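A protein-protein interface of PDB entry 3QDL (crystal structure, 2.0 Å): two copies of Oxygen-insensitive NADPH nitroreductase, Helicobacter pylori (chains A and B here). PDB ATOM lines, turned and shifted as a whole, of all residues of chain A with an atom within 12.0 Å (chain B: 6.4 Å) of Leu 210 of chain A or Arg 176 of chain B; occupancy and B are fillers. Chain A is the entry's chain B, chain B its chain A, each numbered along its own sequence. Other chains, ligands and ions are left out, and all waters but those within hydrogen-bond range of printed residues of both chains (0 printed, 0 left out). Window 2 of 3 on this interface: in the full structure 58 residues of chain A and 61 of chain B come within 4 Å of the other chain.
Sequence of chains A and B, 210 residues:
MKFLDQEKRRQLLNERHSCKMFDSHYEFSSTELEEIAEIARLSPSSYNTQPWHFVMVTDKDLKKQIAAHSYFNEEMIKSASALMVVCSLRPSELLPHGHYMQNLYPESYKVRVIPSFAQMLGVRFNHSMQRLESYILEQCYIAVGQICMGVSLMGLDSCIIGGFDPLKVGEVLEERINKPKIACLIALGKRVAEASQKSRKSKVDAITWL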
ATOM      1  N   LYS A 203     -11.639  -8.010   0.522  1.00  0.00           N
ATOM      2  CA  LYS A 203     -10.736  -8.573  -0.481  1.00  0.00           C
ATOM      3  C   LYS A 203      -9.376  -8.861   0.150  1.00  0.00           C
ATOM      4  O   LYS A 203      -8.715  -9.844  -0.194  1.00  0.00           O
ATOM      5  CB  LYS A 203     -10.584  -7.629  -1.678  1.00  0.00           C
ATOM      6  CG  LYS A 203     -11.893  -7.252  -2.353  1.00  0.00           C
ATOM      7  CD  LYS A 203     -11.675  -6.316  -3.531  1.00  0.00           C
ATOM      8  CE  LYS A 203     -12.975  -5.617  -3.913  1.00  0.00           C
ATOM      9  NZ  LYS A 203     -12.769  -4.572  -4.948  1.00  0.00           N
ATOM     10  N   VAL A 204      -8.984  -8.000   1.089  1.00  0.00           N
ATOM     11  CA  VAL A 204      -7.735  -8.140   1.831  1.00  0.00           C
ATOM     12  C   VAL A 204      -7.730  -9.416   2.681  1.00  0.00           C
ATOM     13  O   VAL A 204      -6.740 -10.151   2.686  1.00  0.00           O
ATOM     14  CB  VAL A 204      -7.446  -6.865   2.674  1.00  0.00           C
ATOM     15  CG1 VAL A 204      -6.452  -7.136   3.797  1.00  0.00           C
ATOM     16  CG2 VAL A 204      -6.942  -5.749   1.765  1.00  0.00           C
ATOM     17  N   ALA A 206      -9.469 -12.010   2.000  1.00  0.00           N
ATOM     18  CA  ALA A 206      -9.690 -13.148   1.107  1.00  0.00           C
ATOM     19  C   ALA A 206      -8.547 -13.458   0.140  1.00  0.00           C
ATOM     20  O   ALA A 206      -8.400 -14.603  -0.295  1.00  0.00           O
ATOM     21  CB  ALA A 206     -10.997 -12.961   0.330  1.00  0.00           C
ATOM     22  N   ILE A 207      -7.749 -12.446  -0.201  1.00  0.00           N
ATOM     23  CA  ILE A 207      -6.755 -12.587  -1.271  1.00  0.00           C
ATOM     24  C   ILE A 207      -5.335 -12.227  -0.832  1.00  0.00           C
ATOM     25  O   ILE A 207      -5.111 -11.174  -0.235  1.00  0.00           O
ATOM     26  CB  ILE A 207      -7.136 -11.729  -2.528  1.00  0.00           C
ATOM     27  CG1 ILE A 207      -8.590 -11.975  -2.968  1.00  0.00           C
ATOM     28  CG2 ILE A 207      -6.159 -11.963  -3.684  1.00  0.00           C
ATOM     29  CD1 ILE A 207      -8.900 -13.396  -3.442  1.00  0.00           C
ATOM     30  N   THR A 208      -4.387 -13.115  -1.133  1.00  0.00           N
ATOM     31  CA  THR A 208      -2.962 -12.796  -1.020  1.00  0.00           C
ATOM     32  C   THR A 208      -2.347 -12.669  -2.414  1.00  0.00           C
ATOM     33  O   THR A 208      -2.409 -13.602  -3.220  1.00  0.00           O
ATOM     34  CB  THR A 208      -2.193 -13.842  -0.179  1.00  0.00           C
ATOM     35  OG1 THR A 208      -2.689 -13.827   1.163  1.00  0.00           O
ATOM     36  CG2 THR A 208      -0.692 -13.540  -0.156  1.00  0.00           C
ATOM     37  N   TRP A 209      -1.760 -11.506  -2.689  1.00  0.00           N
ATOM     38  CA  TRP A 209      -1.160 -11.231  -3.994  1.00  0.00           C
ATOM     39  C   TRP A 209       0.335 -11.521  -4.006  1.00  0.00           C
ATOM     40  O   TRP A 209       1.114 -10.834  -3.341  1.00  0.00           O
ATOM     41  CB  TRP A 209      -1.400  -9.777  -4.407  1.00  0.00           C
ATOM     42  CG  TRP A 209      -2.839  -9.418  -4.611  1.00  0.00           C
ATOM     43  CD1 TRP A 209      -3.640  -8.709  -3.760  1.00  0.00           C
ATOM     44  CD2 TRP A 209      -3.645  -9.735  -5.751  1.00  0.00           C
ATOM     45  NE1 TRP A 209      -4.896  -8.569  -4.298  1.00  0.00           N
ATOM     46  CE2 TRP A 209      -4.928  -9.187  -5.519  1.00  0.00           C
ATOM     47  CE3 TRP A 209      -3.409 -10.429  -6.945  1.00  0.00           C
ATOM     48  CZ2 TRP A 209      -5.976  -9.317  -6.438  1.00  0.00           C
ATOM     49  CZ3 TRP A 209      -4.451 -10.558  -7.859  1.00  0.00           C
ATOM     50  CH2 TRP A 209      -5.720 -10.001  -7.598  1.00  0.00           C
ATOM     51  N   LEU A 210       0.725 -12.540  -4.769  1.00  0.00           N
ATOM     52  CA  LEU A 210       2.133 -12.858  -4.992  1.00  0.00           C
ATOM     53  C   LEU A 210       2.441 -12.827  -6.489  1.00  0.00           C
ATOM     54  O   LEU A 210       1.896 -11.996  -7.217  1.00  0.00           O
ATOM     55  CB  LEU A 210       2.504 -14.221  -4.375  1.00  0.00           C
ATOM     56  CG  LEU A 210       2.349 -14.456  -2.863  1.00  0.00           C
ATOM     57  CD1 LEU A 210       2.945 -15.799  -2.459  1.00  0.00           C
ATOM     58  CD2 LEU A 210       2.948 -13.328  -2.013  1.00  0.00           C
ATOM     59  OXT LEU A 210       3.235 -13.610  -7.018  1.00  0.00           O
ATOM     60  N   VAL B  55      -4.442 -17.613  -2.697  1.00  0.00           N
ATOM     61  CA  VAL B  55      -3.121 -17.026  -2.911  1.00  0.00           C
ATOM     62  C   VAL B  55      -2.811 -17.012  -4.407  1.00  0.00           C
ATOM     63  O   VAL B  55      -2.692 -18.067  -5.030  1.00  0.00           O
ATOM     64  CB  VAL B  55      -2.017 -17.779  -2.123  1.00  0.00           C
ATOM     65  CG1 VAL B  55      -0.652 -17.126  -2.339  1.00  0.00           C
ATOM     66  CG2 VAL B  55      -2.355 -17.825  -0.635  1.00  0.00           C
ATOM     67  N   MET B  56      -2.692 -15.815  -4.973  1.00  0.00           N
ATOM     68  CA  MET B  56      -2.411 -15.657  -6.400  1.00  0.00           C
ATOM     69  C   MET B  56      -0.903 -15.649  -6.646  1.00  0.00           C
ATOM     70  O   MET B  56      -0.218 -14.681  -6.307  1.00  0.00           O
ATOM     71  CB  MET B  56      -3.052 -14.373  -6.952  1.00  0.00           C
ATOM     72  CG  MET B  56      -4.489 -14.124  -6.502  1.00  0.00           C
ATOM     73  SD  MET B  56      -5.683 -15.308  -7.153  1.00  0.00           S
ATOM     74  CE  MET B  56      -5.997 -14.628  -8.778  1.00  0.00           C
ATOM     75  N   VAL B  57      -0.391 -16.729  -7.230  1.00  0.00           N
ATOM     76  CA  VAL B  57       1.041 -16.834  -7.513  1.00  0.00           C
ATOM     77  C   VAL B  57       1.308 -16.527  -8.989  1.00  0.00           C
ATOM     78  O   VAL B  57       0.857 -17.260  -9.874  1.00  0.00           O
ATOM     79  CB  VAL B  57       1.615 -18.227  -7.127  1.00  0.00           C
ATOM     80  CG1 VAL B  57       3.126 -18.281  -7.365  1.00  0.00           C
ATOM     81  CG2 VAL B  57       1.285 -18.570  -5.672  1.00  0.00           C
ATOM     82  N   THR B  58       2.029 -15.435  -9.239  1.00  0.00           N
ATOM     83  CA  THR B  58       2.371 -15.013 -10.602  1.00  0.00           C
ATOM     84  C   THR B  58       3.877 -14.897 -10.841  1.00  0.00           C
ATOM     85  O   THR B  58       4.320 -14.875 -11.990  1.00  0.00           O
ATOM     86  CB  THR B  58       1.713 -13.665 -10.980  1.00  0.00           C
ATOM     87  OG1 THR B  58       2.053 -12.667 -10.009  1.00  0.00           O
ATOM     88  CG2 THR B  58       0.198 -13.802 -11.074  1.00  0.00           C
ATOM     89  N   ASP B  59       4.654 -14.807  -9.761  1.00  0.00           N
ATOM     90  CA  ASP B  59       6.114 -14.765  -9.856  1.00  0.00           C
ATOM     91  C   ASP B  59       6.637 -16.091 -10.398  1.00  0.00           C
ATOM     92  O   ASP B  59       6.338 -17.154  -9.840  1.00  0.00           O
ATOM     93  CB  ASP B  59       6.733 -14.459  -8.489  1.00  0.00           C
ATOM     94  CG  ASP B  59       8.235 -14.269  -8.560  1.00  0.00           C
ATOM     95  OD1 ASP B  59       8.680 -13.106  -8.497  1.00  0.00           O
ATOM     96  OD2 ASP B  59       8.970 -15.272  -8.692  1.00  0.00           O
ATOM     97  N   LEU B  62       8.859 -18.351  -8.088  1.00  0.00           N
ATOM     98  CA  LEU B  62       8.041 -18.832  -6.981  1.00  0.00           C
ATOM     99  C   LEU B  62       7.081 -19.930  -7.448  1.00  0.00           C
ATOM    100  O   LEU B  62       6.900 -20.940  -6.764  1.00  0.00           O
ATOM    101  CB  LEU B  62       7.273 -17.663  -6.356  1.00  0.00           C
ATOM    102  CG  LEU B  62       6.687 -17.812  -4.950  1.00  0.00           C
ATOM    103  CD1 LEU B  62       7.746 -18.219  -3.925  1.00  0.00           C
ATOM    104  CD2 LEU B  62       6.021 -16.510  -4.538  1.00  0.00           C
ATOM    105  N   VAL B 172       8.113 -24.116   0.415  1.00  0.00           N
ATOM    106  CA  VAL B 172       8.541 -23.000  -0.441  1.00  0.00           C
ATOM    107  C   VAL B 172       7.608 -21.785  -0.392  1.00  0.00           C
ATOM    108  O   VAL B 172       7.851 -20.780  -1.067  1.00  0.00           O
ATOM    109  CB  VAL B 172       8.784 -23.444  -1.914  1.00  0.00           C
ATOM    110  CG1 VAL B 172       9.964 -24.407  -1.997  1.00  0.00           C
ATOM    111  CG2 VAL B 172       7.531 -24.065  -2.523  1.00  0.00           C
ATOM    112  N   LEU B 173       6.551 -21.881   0.411  1.00  0.00           N
ATOM    113  CA  LEU B 173       5.618 -20.771   0.610  1.00  0.00           C
ATOM    114  C   LEU B 173       5.567 -20.321   2.071  1.00  0.00           C
ATOM    115  O   LEU B 173       4.831 -19.393   2.415  1.00  0.00           O
ATOM    116  CB  LEU B 173       4.216 -21.149   0.115  1.00  0.00           C
ATOM    117  CG  LEU B 173       3.962 -21.202  -1.396  1.00  0.00           C
ATOM    118  CD1 LEU B 173       2.676 -21.962  -1.691  1.00  0.00           C
ATOM    119  CD2 LEU B 173       3.917 -19.804  -2.020  1.00  0.00           C
ATOM    120  N   GLU B 174       6.364 -20.976   2.914  1.00  0.00           N
ATOM    121  CA  GLU B 174       6.374 -20.735   4.362  1.00  0.00           C
ATOM    122  C   GLU B 174       6.840 -19.340   4.783  1.00  0.00           C
ATOM    123  O   GLU B 174       6.131 -18.640   5.507  1.00  0.00           O
ATOM    124  CB  GLU B 174       7.217 -21.792   5.079  1.00  0.00           C
ATOM    125  CG  GLU B 174       6.411 -22.944   5.643  1.00  0.00           C
ATOM    126  CD  GLU B 174       7.126 -23.649   6.777  1.00  0.00           C
ATOM    127  OE1 GLU B 174       8.256 -24.140   6.563  1.00  0.00           O
ATOM    128  OE2 GLU B 174       6.551 -23.712   7.884  1.00  0.00           O
ATOM    129  N   GLU B 175       8.033 -18.950   4.336  1.00  0.00           N
ATOM    130  CA  GLU B 175       8.628 -17.662   4.709  1.00  0.00           C
ATOM    131  C   GLU B 175       7.807 -16.478   4.193  1.00  0.00           C
ATOM    132  O   GLU B 175       7.883 -15.373   4.736  1.00  0.00           O
ATOM    133  CB  GLU B 175      10.082 -17.568   4.221  1.00  0.00           C
ATOM    134  CG  GLU B 175      10.260 -17.296   2.719  1.00  0.00           C
ATOM    135  CD  GLU B 175      10.254 -18.553   1.858  1.00  0.00           C
ATOM    136  OE1 GLU B 175       9.512 -19.512   2.168  1.00  0.00           O
ATOM    137  OE2 GLU B 175      10.995 -18.572   0.852  1.00  0.00           O
ATOM    138  N   ARG B 176       7.020 -16.736   3.151  1.00  0.00           N
ATOM    139  CA  ARG B 176       6.197 -15.722   2.514  1.00  0.00           C
ATOM    140  C   ARG B 176       4.874 -15.542   3.260  1.00  0.00           C
ATOM    141  O   ARG B 176       4.447 -14.415   3.516  1.00  0.00           O
ATOM    142  CB  ARG B 176       5.962 -16.096   1.044  1.00  0.00           C
ATOM    143  CG  ARG B 176       5.627 -14.930   0.135  1.00  0.00           C
ATOM    144  CD  ARG B 176       6.705 -13.845   0.161  1.00  0.00           C
ATOM    145  NE  ARG B 176       6.186 -12.564  -0.320  1.00  0.00           N
ATOM    146  CZ  ARG B 176       5.401 -11.755   0.388  1.00  0.00           C
ATOM    147  NH1 ARG B 176       5.031 -12.084   1.620  1.00  0.00           N
ATOM    148  NH2 ARG B 176       4.979 -10.613  -0.139  1.00  0.00           N
ATOM    149  N   ILE B 177       4.238 -16.658   3.610  1.00  0.00           N
ATOM    150  CA  ILE B 177       3.002 -16.652   4.397  1.00  0.00           C
ATOM    151  C   ILE B 177       2.982 -17.808   5.396  1.00  0.00           C
ATOM    152  O   ILE B 177       3.585 -18.857   5.152  1.00  0.00           O
ATOM    153  CB  ILE B 177       1.725 -16.703   3.506  1.00  0.00           C
ATOM    154  CG1 ILE B 177       1.912 -17.643   2.310  1.00  0.00           C
ATOM    155  CG2 ILE B 177       1.337 -15.310   3.029  1.00  0.00           C
ATOM    156  CD1 ILE B 177       1.393 -19.050   2.535  1.00  0.00           C
ATOM    157  N   ASN B 178       2.284 -17.610   6.514  1.00  0.00           N
ATOM    158  CA  ASN B 178       2.119 -18.650   7.532  1.00  0.00           C
ATOM    159  C   ASN B 178       1.718 -19.979   6.905  1.00  0.00           C
ATOM    160  O   ASN B 178       0.905 -20.006   5.975  1.00  0.00           O
ATOM    161  CB  ASN B 178       1.075 -18.227   8.565  1.00  0.00           C
ATOM    162  CG  ASN B 178       1.479 -16.981   9.323  1.00  0.00           C
ATOM    163  OD1 ASN B 178       2.373 -17.014  10.166  1.00  0.00           O
ATOM    164  ND2 ASN B 178       0.818 -15.870   9.025  1.00  0.00           N
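Ile 207 of chain A touches Met 56 of chain B. Val 55 of chain B touches Thr 208 of chain A. CG of Met 56 of chain B touches CZ3 of Trp 209 of chain A, 3.8 Å away. CG1 of Val 55 of chain B touches CD1 of Leu 210 of chain A, 3.8 Å away. Val 57 of chain B touches Leu 210 of chain A (CA to OXT, 3.9 Å). Leu 210 of chain A touches Leu 62 of chain B. CD2 of Leu 210 of chain A touches NE of Arg 176 of chain B, 3.7 Å away.
Lys 203 of chain A touches none of the printed residues of chain B. Printed residues of chain B within 4 Å of Ile 207 of chain A: Met 56 (3.9 Å). Of the printed residues of chain B, Thr 208 of chain A touches Val 55 (3.5 Å) and Met 56 (2.8 Å). Of chain B, only Val 55 (3.8 Å), Met 56 (2.8 Å), Val 57 (3.9 Å), Thr 58 (2.9 Å), Asp 59 (3.3 Å), Leu 62 (3.8 Å) and Arg 176 (3.7 Å) come within 4 Å of Leu 210 of chain A. Val 55 of chain B touches just these residues of chain A: Thr 208 (3.5 Å) and Leu 210 (3.8 Å). Of the printed residues of chain A, Met 56 of chain B touches Ile 207, Thr 208, Trp 209 and Leu 210. Of the printed residues of chain A, Val 57 of chain B touches Leu 210. Of chain A, only Leu 210 (3.3 Å) comes within 4 Å of Asp 59 of chain B. Leu 62 of chain B touches just one residue of chain A: Leu 210. Val 172 of chain B touches none of the printed residues of chain A. No residue of chain A comes within 4 Å of Leu 173 of chain B. No residue of chain A comes within 4 Å of Glu 175 of chain B. Of chain A, only Leu 210 (3.7 Å) comes within 4 Å of Arg 176 of chain B. No residue of chain A comes within 4 Å of Ile 177 of chain B. Asn 178 of chain B touches none of the printed residues of chain A. The nearest residue of chain B that does not touch Leu 210 of chain A is Leu 173 of chain B (4.1 Å). The nearest printed residue of chain B that does not touch Thr 208 of chain A is Ile 177 of chain B (4.2 Å).
Hydrophobic or aromatic side chains of chain A within 4 Å of the printed part of chain B: Ile 207, Trp 209 and Leu 210. Of the 13 printed residues of chain B, 7 touch a printed residue of chain A. Hydrophobic or aromatic side chains of chain B within 4 Å of the printed part of chain A: Val 55, Met 56 and Leu 62. Along chain B the printed residues that touch a printed residue of chain A span positions 55 to 176. Among the printed residues, no Asp or Glu carboxylate lies within 4 Å of a Lys or Arg side-chain nitrogen of the other chain.
N of Met 56 of chain B lies within hydrogen-bond range of O of Thr 208 of chain A, at 2.8 Å. The backbone carbonyl oxygen (O) of Met 56 of chain B is in hydrogen-bond range of the backbone NH (N) of Leu 210 of chain A (2.8 Å). The side-chain hydroxyl of Thr 58 of chain B lies within hydrogen-bond range of the chain-end carboxylate of Leu 210 of chain A. The backbone NH (N) of Asp 59 of chain B lies within hydrogen-bond range of the chain-end carboxylate (OXT) of Leu 210 of chain A (3.3 Å).
No position is printed for both chains. Of the 11 pairs that touch across the chains among the printed residues, none has its exchanged pair printed and touching as well.
The side-chain carboxylate (OD2) of Asp 59 of chain B sits at hydrogen-bond distance from the backbone NH (N) of Leu 62 of chain B (3.1 Å).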
